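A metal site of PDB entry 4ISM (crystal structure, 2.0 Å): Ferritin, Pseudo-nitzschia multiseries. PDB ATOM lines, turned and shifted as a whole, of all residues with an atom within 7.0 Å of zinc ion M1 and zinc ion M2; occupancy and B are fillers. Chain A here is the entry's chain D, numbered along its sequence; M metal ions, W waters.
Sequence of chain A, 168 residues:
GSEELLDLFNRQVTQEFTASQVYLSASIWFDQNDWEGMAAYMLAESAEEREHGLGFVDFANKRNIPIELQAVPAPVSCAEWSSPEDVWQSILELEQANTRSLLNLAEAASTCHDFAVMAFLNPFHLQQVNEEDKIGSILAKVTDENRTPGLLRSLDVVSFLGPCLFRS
The side-chain amide nitrogen of Asn 98 is in hydrogen-bond range of the side-chain carboxylate of Glu 16. The side-chain carboxylate (OE2) of Glu 16 lies within hydrogen-bond range of the side-chain amide nitrogen (NE2) of Gln 12 (2.9 Å). O of Glu 95 sits at hydrogen-bond distance from NE2 of Gln 128 (3.1 Å). The side-chain carboxylate (OE2) of Glu 95 lies close to the side-chain hydroxyl (OH) of Tyr 23 (2.5 Å). The side-chain amide oxygen of Asn 98 is in hydrogen-bond range of the side-chain amide nitrogen of Gln 12 (3.0 Å).
Asn 98 touches zinc ion M1 (ND2 to ZN, 3.3 Å). Within 4 Å of zinc ion M1: Glu 16, Glu 49, His 52 and Asn 98. The nearest printed residue that does not touch zinc ion M1 is Gln 128 (4.2 Å).
Gln 128 touches zinc ion M2 (OE1 to ZN, 3.7 Å). Three residues have an atom within 4 Å of zinc ion M2: Glu 49, Glu 95 and Gln 128.
Zinc ion M1 is bound by the side-chain carboxylate (OE1) of Glu 16 (2.0 Å), water W1 (2.1 Å), a ring nitrogen (ND1) of His 52 (2.1 Å), the side-chain carboxylate (OE1) of Glu 49 (2.1 Å) and water W2 (2.3 Å).
Zinc ion M2 is bound by OE2 of Glu 49, water W1, OE2 of Glu 95 and OE1 of Glu 95. Zinc ion M2 has four donor atoms within binding distance. Slightly farther from zinc ion M2 lies water W3 (2.7 Å).
Water W1 bridges the side-chain amide oxygen of Gln 128 (2.7 Å) and the side-chain amide nitrogen of Asn 98 (3.0 Å). Water W2 lies within hydrogen-bond range of the side-chain carboxylate (OE2) of Glu 16 (2.6 Å) and the side-chain amide nitrogen (ND2) of Asn 98 (3.2 Å).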
ATOM      1  N   GLN A  12     -22.629  15.737  16.077  1.00  0.00           N
ATOM      2  CA  GLN A  12     -21.243  15.134  16.020  1.00  0.00           C
ATOM      3  C   GLN A  12     -20.617  15.424  14.661  1.00  0.00           C
ATOM      4  O   GLN A  12     -19.389  15.630  14.577  1.00  0.00           O
ATOM      5  CB  GLN A  12     -21.316  13.639  16.263  1.00  0.00           C
ATOM      6  CG  GLN A  12     -19.941  13.018  16.563  1.00  0.00           C
ATOM      7  CD  GLN A  12     -19.213  13.679  17.714  1.00  0.00           C
ATOM      8  OE1 GLN A  12     -19.826  14.100  18.719  1.00  0.00           O
ATOM      9  NE2 GLN A  12     -17.902  13.775  17.571  1.00  0.00           N
ATOM     10  N   GLN A  15     -19.138  18.804  14.870  1.00  0.00           N
ATOM     11  CA  GLN A  15     -17.923  18.814  15.652  1.00  0.00           C
ATOM     12  C   GLN A  15     -16.726  18.255  14.868  1.00  0.00           C
ATOM     13  O   GLN A  15     -15.635  18.803  14.999  1.00  0.00           O
ATOM     14  CB  GLN A  15     -18.122  17.971  16.903  1.00  0.00           C
ATOM     15  CG  GLN A  15     -16.860  18.003  17.722  1.00  0.00           C
ATOM     16  CD  GLN A  15     -16.903  19.032  18.853  1.00  0.00           C
ATOM     17  OE1 GLN A  15     -17.466  20.168  18.703  1.00  0.00           O
ATOM     18  NE2 GLN A  15     -16.399  18.594  20.045  1.00  0.00           N
ATOM     19  N   GLU A  16     -16.908  17.171  14.079  1.00  0.00           N
ATOM     20  CA  GLU A  16     -15.739  16.605  13.358  1.00  0.00           C
ATOM     21  C   GLU A  16     -15.324  17.646  12.307  1.00  0.00           C
ATOM     22  O   GLU A  16     -14.131  17.911  12.124  1.00  0.00           O
ATOM     23  CB  GLU A  16     -16.091  15.272  12.667  1.00  0.00           C
ATOM     24  CG  GLU A  16     -16.614  14.182  13.640  1.00  0.00           C
ATOM     25  CD  GLU A  16     -15.498  13.709  14.570  1.00  0.00           C
ATOM     26  OE1 GLU A  16     -14.286  13.936  14.242  1.00  0.00           O
ATOM     27  OE2 GLU A  16     -15.806  13.182  15.663  1.00  0.00           O
ATOM     28  N   ALA A  19     -13.488  20.581  13.943  1.00  0.00           N
ATOM     29  CA  ALA A  19     -12.134  20.080  14.239  1.00  0.00           C
ATOM     30  C   ALA A  19     -11.316  20.097  12.995  1.00  0.00           C
ATOM     31  O   ALA A  19     -10.166  20.549  13.016  1.00  0.00           O
ATOM     32  CB  ALA A  19     -12.180  18.654  14.897  1.00  0.00           C
ATOM     33  N   TYR A  23      -7.800  22.239  12.786  1.00  0.00           N
ATOM     34  CA  TYR A  23      -6.482  21.684  12.261  1.00  0.00           C
ATOM     35  C   TYR A  23      -6.028  22.414  11.038  1.00  0.00           C
ATOM     36  O   TYR A  23      -4.870  22.721  10.971  1.00  0.00           O
ATOM     37  CB  TYR A  23      -6.655  20.201  11.889  1.00  0.00           C
ATOM     38  CG  TYR A  23      -6.523  19.327  13.114  1.00  0.00           C
ATOM     39  CD1 TYR A  23      -7.619  18.729  13.703  1.00  0.00           C
ATOM     40  CD2 TYR A  23      -5.248  19.075  13.678  1.00  0.00           C
ATOM     41  CE1 TYR A  23      -7.482  17.846  14.815  1.00  0.00           C
ATOM     42  CE2 TYR A  23      -5.119  18.193  14.762  1.00  0.00           C
ATOM     43  CZ  TYR A  23      -6.228  17.582  15.309  1.00  0.00           C
ATOM     44  OH  TYR A  23      -6.074  16.746  16.425  1.00  0.00           O
ATOM     45  N   GLU A  45      -4.061  15.746   9.761  1.00  0.00           N
ATOM     46  CA  GLU A  45      -5.081  15.619  10.735  1.00  0.00           C
ATOM     47  C   GLU A  45      -6.362  16.306  10.349  1.00  0.00           C
ATOM     48  O   GLU A  45      -7.487  15.846  10.692  1.00  0.00           O
ATOM     49  CB  GLU A  45      -4.648  16.153  12.118  1.00  0.00           C
ATOM     50  CG  GLU A  45      -3.642  15.229  12.788  1.00  0.00           C
ATOM     51  CD  GLU A  45      -4.346  13.923  13.130  1.00  0.00           C
ATOM     52  OE1 GLU A  45      -5.552  13.963  13.530  1.00  0.00           O
ATOM     53  OE2 GLU A  45      -3.736  12.856  12.964  1.00  0.00           O
ATOM     54  N   GLU A  48      -8.166  13.879   8.120  1.00  0.00           N
ATOM     55  CA  GLU A  48      -8.673  12.795   8.916  1.00  0.00           C
ATOM     56  C   GLU A  48      -9.951  13.156   9.684  1.00  0.00           C
ATOM     57  O   GLU A  48     -10.850  12.278   9.835  1.00  0.00           O
ATOM     58  CB  GLU A  48      -7.610  12.400   9.930  1.00  0.00           C
ATOM     59  CG  GLU A  48      -8.073  11.366  10.943  1.00  0.00           C
ATOM     60  CD  GLU A  48      -6.979  11.149  11.980  1.00  0.00           C
ATOM     61  OE1 GLU A  48      -5.800  10.916  11.588  1.00  0.00           O
ATOM     62  OE2 GLU A  48      -7.283  11.283  13.184  1.00  0.00           O
ATOM     63  N   GLU A  49     -10.009  14.358  10.254  1.00  0.00           N
ATOM     64  CA  GLU A  49     -11.242  14.744  10.965  1.00  0.00           C
ATOM     65  C   GLU A  49     -12.362  14.808   9.982  1.00  0.00           C
ATOM     66  O   GLU A  49     -13.553  14.491  10.311  1.00  0.00           O
ATOM     67  CB  GLU A  49     -11.089  16.139  11.635  1.00  0.00           C
ATOM     68  CG  GLU A  49     -10.101  16.156  12.784  1.00  0.00           C
ATOM     69  CD  GLU A  49     -10.502  15.229  13.919  1.00  0.00           C
ATOM     70  OE1 GLU A  49     -11.674  14.890  14.024  1.00  0.00           O
ATOM     71  OE2 GLU A  49      -9.650  14.727  14.677  1.00  0.00           O
ATOM     72  N   ARG A  50     -12.058  15.299   8.778  1.00  0.00           N
ATOM     73  CA  ARG A  50     -13.078  15.280   7.763  1.00  0.00           C
ATOM     74  C   ARG A  50     -13.591  13.851   7.499  1.00  0.00           C
ATOM     75  O   ARG A  50     -14.812  13.612   7.451  1.00  0.00           O
ATOM     76  CB  ARG A  50     -12.641  16.002   6.446  1.00  0.00           C
ATOM     77  CG  ARG A  50     -13.755  16.046   5.422  1.00  0.00           C
ATOM     78  CD  ARG A  50     -13.634  17.196   4.407  1.00  0.00           C
ATOM     79  NE  ARG A  50     -14.720  17.200   3.387  1.00  0.00           N
ATOM     80  CZ  ARG A  50     -14.710  16.312   2.386  1.00  0.00           C
ATOM     81  NH1 ARG A  50     -13.728  15.479   2.345  1.00  0.00           N
ATOM     82  NH2 ARG A  50     -15.681  16.194   1.522  1.00  0.00           N
ATOM     83  N   HIS A  52     -13.624  11.394   9.530  1.00  0.00           N
ATOM     84  CA  HIS A  52     -14.492  11.013  10.688  1.00  0.00           C
ATOM     85  C   HIS A  52     -15.926  11.550  10.512  1.00  0.00           C
ATOM     86  O   HIS A  52     -16.891  10.839  10.775  1.00  0.00           O
ATOM     87  CB  HIS A  52     -14.009  11.596  12.061  1.00  0.00           C
ATOM     88  CG  HIS A  52     -12.665  11.101  12.520  1.00  0.00           C
ATOM     89  ND1 HIS A  52     -11.970  11.727  13.523  1.00  0.00           N
ATOM     90  CD2 HIS A  52     -11.874  10.073  12.103  1.00  0.00           C
ATOM     91  CE1 HIS A  52     -10.800  11.133  13.691  1.00  0.00           C
ATOM     92  NE2 HIS A  52     -10.702  10.132  12.830  1.00  0.00           N
ATOM     93  N   GLY A  53     -16.043  12.831  10.200  1.00  0.00           N
ATOM     94  CA  GLY A  53     -17.371  13.406   9.920  1.00  0.00           C
ATOM     95  C   GLY A  53     -18.120  12.614   8.843  1.00  0.00           C
ATOM     96  O   GLY A  53     -19.349  12.379   8.929  1.00  0.00           O
ATOM     97  N   PHE A  56     -19.634   9.473  10.169  1.00  0.00           N
ATOM     98  CA  PHE A  56     -20.867   9.736  10.862  1.00  0.00           C
ATOM     99  C   PHE A  56     -21.992   9.999   9.891  1.00  0.00           C
ATOM    100  O   PHE A  56     -23.112   9.458  10.063  1.00  0.00           O
ATOM    101  CB  PHE A  56     -20.723  10.929  11.832  1.00  0.00           C
ATOM    102  CG  PHE A  56     -20.133  10.490  13.148  1.00  0.00           C
ATOM    103  CD1 PHE A  56     -18.737  10.279  13.268  1.00  0.00           C
ATOM    104  CD2 PHE A  56     -20.965  10.167  14.246  1.00  0.00           C
ATOM    105  CE1 PHE A  56     -18.184   9.800  14.458  1.00  0.00           C
ATOM    106  CE2 PHE A  56     -20.381   9.685  15.431  1.00  0.00           C
ATOM    107  CZ  PHE A  56     -19.001   9.517  15.539  1.00  0.00           C
ATOM    108  N   LEU A  94      -9.012  20.863  21.689  1.00  0.00           N
ATOM    109  CA  LEU A  94      -9.952  20.465  20.636  1.00  0.00           C
ATOM    110  C   LEU A  94     -10.225  18.923  20.767  1.00  0.00           C
ATOM    111  O   LEU A  94     -11.355  18.453  20.685  1.00  0.00           O
ATOM    112  CB  LEU A  94      -9.337  20.811  19.265  1.00  0.00           C
ATOM    113  CG  LEU A  94     -10.099  20.308  18.029  1.00  0.00           C
ATOM    114  CD1 LEU A  94     -11.353  21.183  17.913  1.00  0.00           C
ATOM    115  CD2 LEU A  94      -9.216  20.473  16.769  1.00  0.00           C
ATOM    116  N   GLU A  95      -9.180  18.115  20.876  1.00  0.00           N
ATOM    117  CA  GLU A  95      -9.420  16.655  20.953  1.00  0.00           C
ATOM    118  C   GLU A  95     -10.111  16.255  22.226  1.00  0.00           C
ATOM    119  O   GLU A  95     -10.942  15.358  22.225  1.00  0.00           O
ATOM    120  CB  GLU A  95      -8.134  15.880  20.828  1.00  0.00           C
ATOM    121  CG  GLU A  95      -7.555  15.884  19.447  1.00  0.00           C
ATOM    122  CD  GLU A  95      -8.462  15.250  18.400  1.00  0.00           C
ATOM    123  OE1 GLU A  95      -9.453  14.536  18.719  1.00  0.00           O
ATOM    124  OE2 GLU A  95      -8.116  15.449  17.228  1.00  0.00           O
ATOM    125  N   ASN A  98     -13.593  16.893  21.578  1.00  0.00           N
ATOM    126  CA  ASN A  98     -14.214  15.923  20.790  1.00  0.00           C
ATOM    127  C   ASN A  98     -14.411  14.584  21.477  1.00  0.00           C
ATOM    128  O   ASN A  98     -15.367  13.881  21.215  1.00  0.00           O
ATOM    129  CB  ASN A  98     -13.516  15.718  19.523  1.00  0.00           C
ATOM    130  CG  ASN A  98     -14.427  15.151  18.570  1.00  0.00           C
ATOM    131  OD1 ASN A  98     -15.633  15.456  18.650  1.00  0.00           O
ATOM    132  ND2 ASN A  98     -13.959  14.265  17.723  1.00  0.00           N
ATOM    133  N   LEU A 102     -18.094  12.614  21.914  1.00  0.00           N
ATOM    134  CA  LEU A 102     -18.372  11.233  21.586  1.00  0.00           C
ATOM    135  C   LEU A 102     -18.919  10.485  22.828  1.00  0.00           C
ATOM    136  O   LEU A 102     -19.823   9.629  22.701  1.00  0.00           O
ATOM    137  CB  LEU A 102     -17.108  10.533  21.099  1.00  0.00           C
ATOM    138  CG  LEU A 102     -16.760  11.110  19.698  1.00  0.00           C
ATOM    139  CD1 LEU A 102     -15.290  10.784  19.390  1.00  0.00           C
ATOM    140  CD2 LEU A 102     -17.713  10.549  18.615  1.00  0.00           C
ATOM    141  N   PHE A 124     -14.235   4.816  17.536  1.00  0.00           N
ATOM    142  CA  PHE A 124     -13.975   6.262  17.709  1.00  0.00           C
ATOM    143  C   PHE A 124     -13.550   6.516  19.142  1.00  0.00           C
ATOM    144  O   PHE A 124     -12.688   7.332  19.342  1.00  0.00           O
ATOM    145  CB  PHE A 124     -15.224   7.137  17.366  1.00  0.00           C
ATOM    146  CG  PHE A 124     -15.538   7.127  15.905  1.00  0.00           C
ATOM    147  CD1 PHE A 124     -14.863   7.981  15.036  1.00  0.00           C
ATOM    148  CD2 PHE A 124     -16.434   6.182  15.374  1.00  0.00           C
ATOM    149  CE1 PHE A 124     -15.113   7.932  13.673  1.00  0.00           C
ATOM    150  CE2 PHE A 124     -16.660   6.109  13.999  1.00  0.00           C
ATOM    151  CZ  PHE A 124     -16.000   6.983  13.142  1.00  0.00           C
ATOM    152  N   GLN A 127     -10.002   5.478  19.100  1.00  0.00           N
ATOM    153  CA  GLN A 127      -9.180   6.466  18.340  1.00  0.00           C
ATOM    154  C   GLN A 127      -8.852   7.676  19.217  1.00  0.00           C
ATOM    155  O   GLN A 127      -7.683   8.100  19.262  1.00  0.00           O
ATOM    156  CB  GLN A 127      -9.879   6.931  17.045  1.00  0.00           C
ATOM    157  CG  GLN A 127      -9.337   8.242  16.460  1.00  0.00           C
ATOM    158  CD  GLN A 127      -8.144   8.010  15.579  1.00  0.00           C
ATOM    159  OE1 GLN A 127      -7.665   6.890  15.496  1.00  0.00           O
ATOM    160  NE2 GLN A 127      -7.653   9.070  14.905  1.00  0.00           N
ATOM    161  N   GLN A 128      -9.863   8.228  19.889  1.00  0.00           N
ATOM    162  CA  GLN A 128      -9.686   9.411  20.783  1.00  0.00           C
ATOM    163  C   GLN A 128      -8.664   9.177  21.861  1.00  0.00           C
ATOM    164  O   GLN A 128      -7.821  10.041  22.120  1.00  0.00           O
ATOM    165  CB  GLN A 128     -11.026   9.819  21.474  1.00  0.00           C
ATOM    166  CG  GLN A 128     -12.027  10.501  20.582  1.00  0.00           C
ATOM    167  CD  GLN A 128     -11.398  11.663  19.814  1.00  0.00           C
ATOM    168  OE1 GLN A 128     -11.224  11.585  18.621  1.00  0.00           O
ATOM    169  NE2 GLN A 128     -10.954  12.694  20.547  1.00  0.00           N
ATOM    170  N   GLU A 131      -5.357   9.512  19.996  1.00  0.00           N
ATOM    171  CA  GLU A 131      -5.090  10.887  19.551  1.00  0.00           C
ATOM    172  C   GLU A 131      -4.689  11.765  20.720  1.00  0.00           C
ATOM    173  O   GLU A 131      -3.699  12.524  20.638  1.00  0.00           O
ATOM    174  CB  GLU A 131      -6.304  11.524  18.880  1.00  0.00           C
ATOM    175  CG  GLU A 131      -5.877  12.702  18.039  1.00  0.00           C
ATOM    176  CD  GLU A 131      -5.307  12.246  16.708  1.00  0.00           C
ATOM    177  OE1 GLU A 131      -6.042  11.562  15.992  1.00  0.00           O
ATOM    178  OE2 GLU A 131      -4.127  12.537  16.395  1.00  0.00           O
ATOM    179  N   ILE A 135      -1.048  13.645  21.012  1.00  0.00           N
ATOM    180  CA  ILE A 135      -0.944  15.130  21.027  1.00  0.00           C
ATOM    181  C   ILE A 135      -0.319  15.528  22.314  1.00  0.00           C
ATOM    182  O   ILE A 135       0.516  16.441  22.342  1.00  0.00           O
ATOM    183  CB  ILE A 135      -2.324  15.852  20.860  1.00  0.00           C
ATOM    184  CG1 ILE A 135      -2.729  15.712  19.420  1.00  0.00           C
ATOM    185  CG2 ILE A 135      -2.288  17.359  21.190  1.00  0.00           C
ATOM    186  CD1 ILE A 135      -4.220  15.667  19.352  1.00  0.00           C
HETATM  187 ZN    ZN M   1     -12.570  13.154  14.910  1.00  0.00          ZN
HETATM  188 ZN    ZN M   2      -9.607  13.978  16.293  1.00  0.00          ZN
HETATM  189 ZN    ZN M   3      -5.121  11.437  13.933  1.00  0.00          ZN
HETATM  190  O   HOH W   1     -11.370  13.361  16.586  1.00  0.00           O
HETATM  191  O   HOH W   2     -13.816  11.561  16.055  1.00  0.00           O
HETATM  192  O   HOH W   3      -7.619  13.581  14.479  1.00  0.00           O
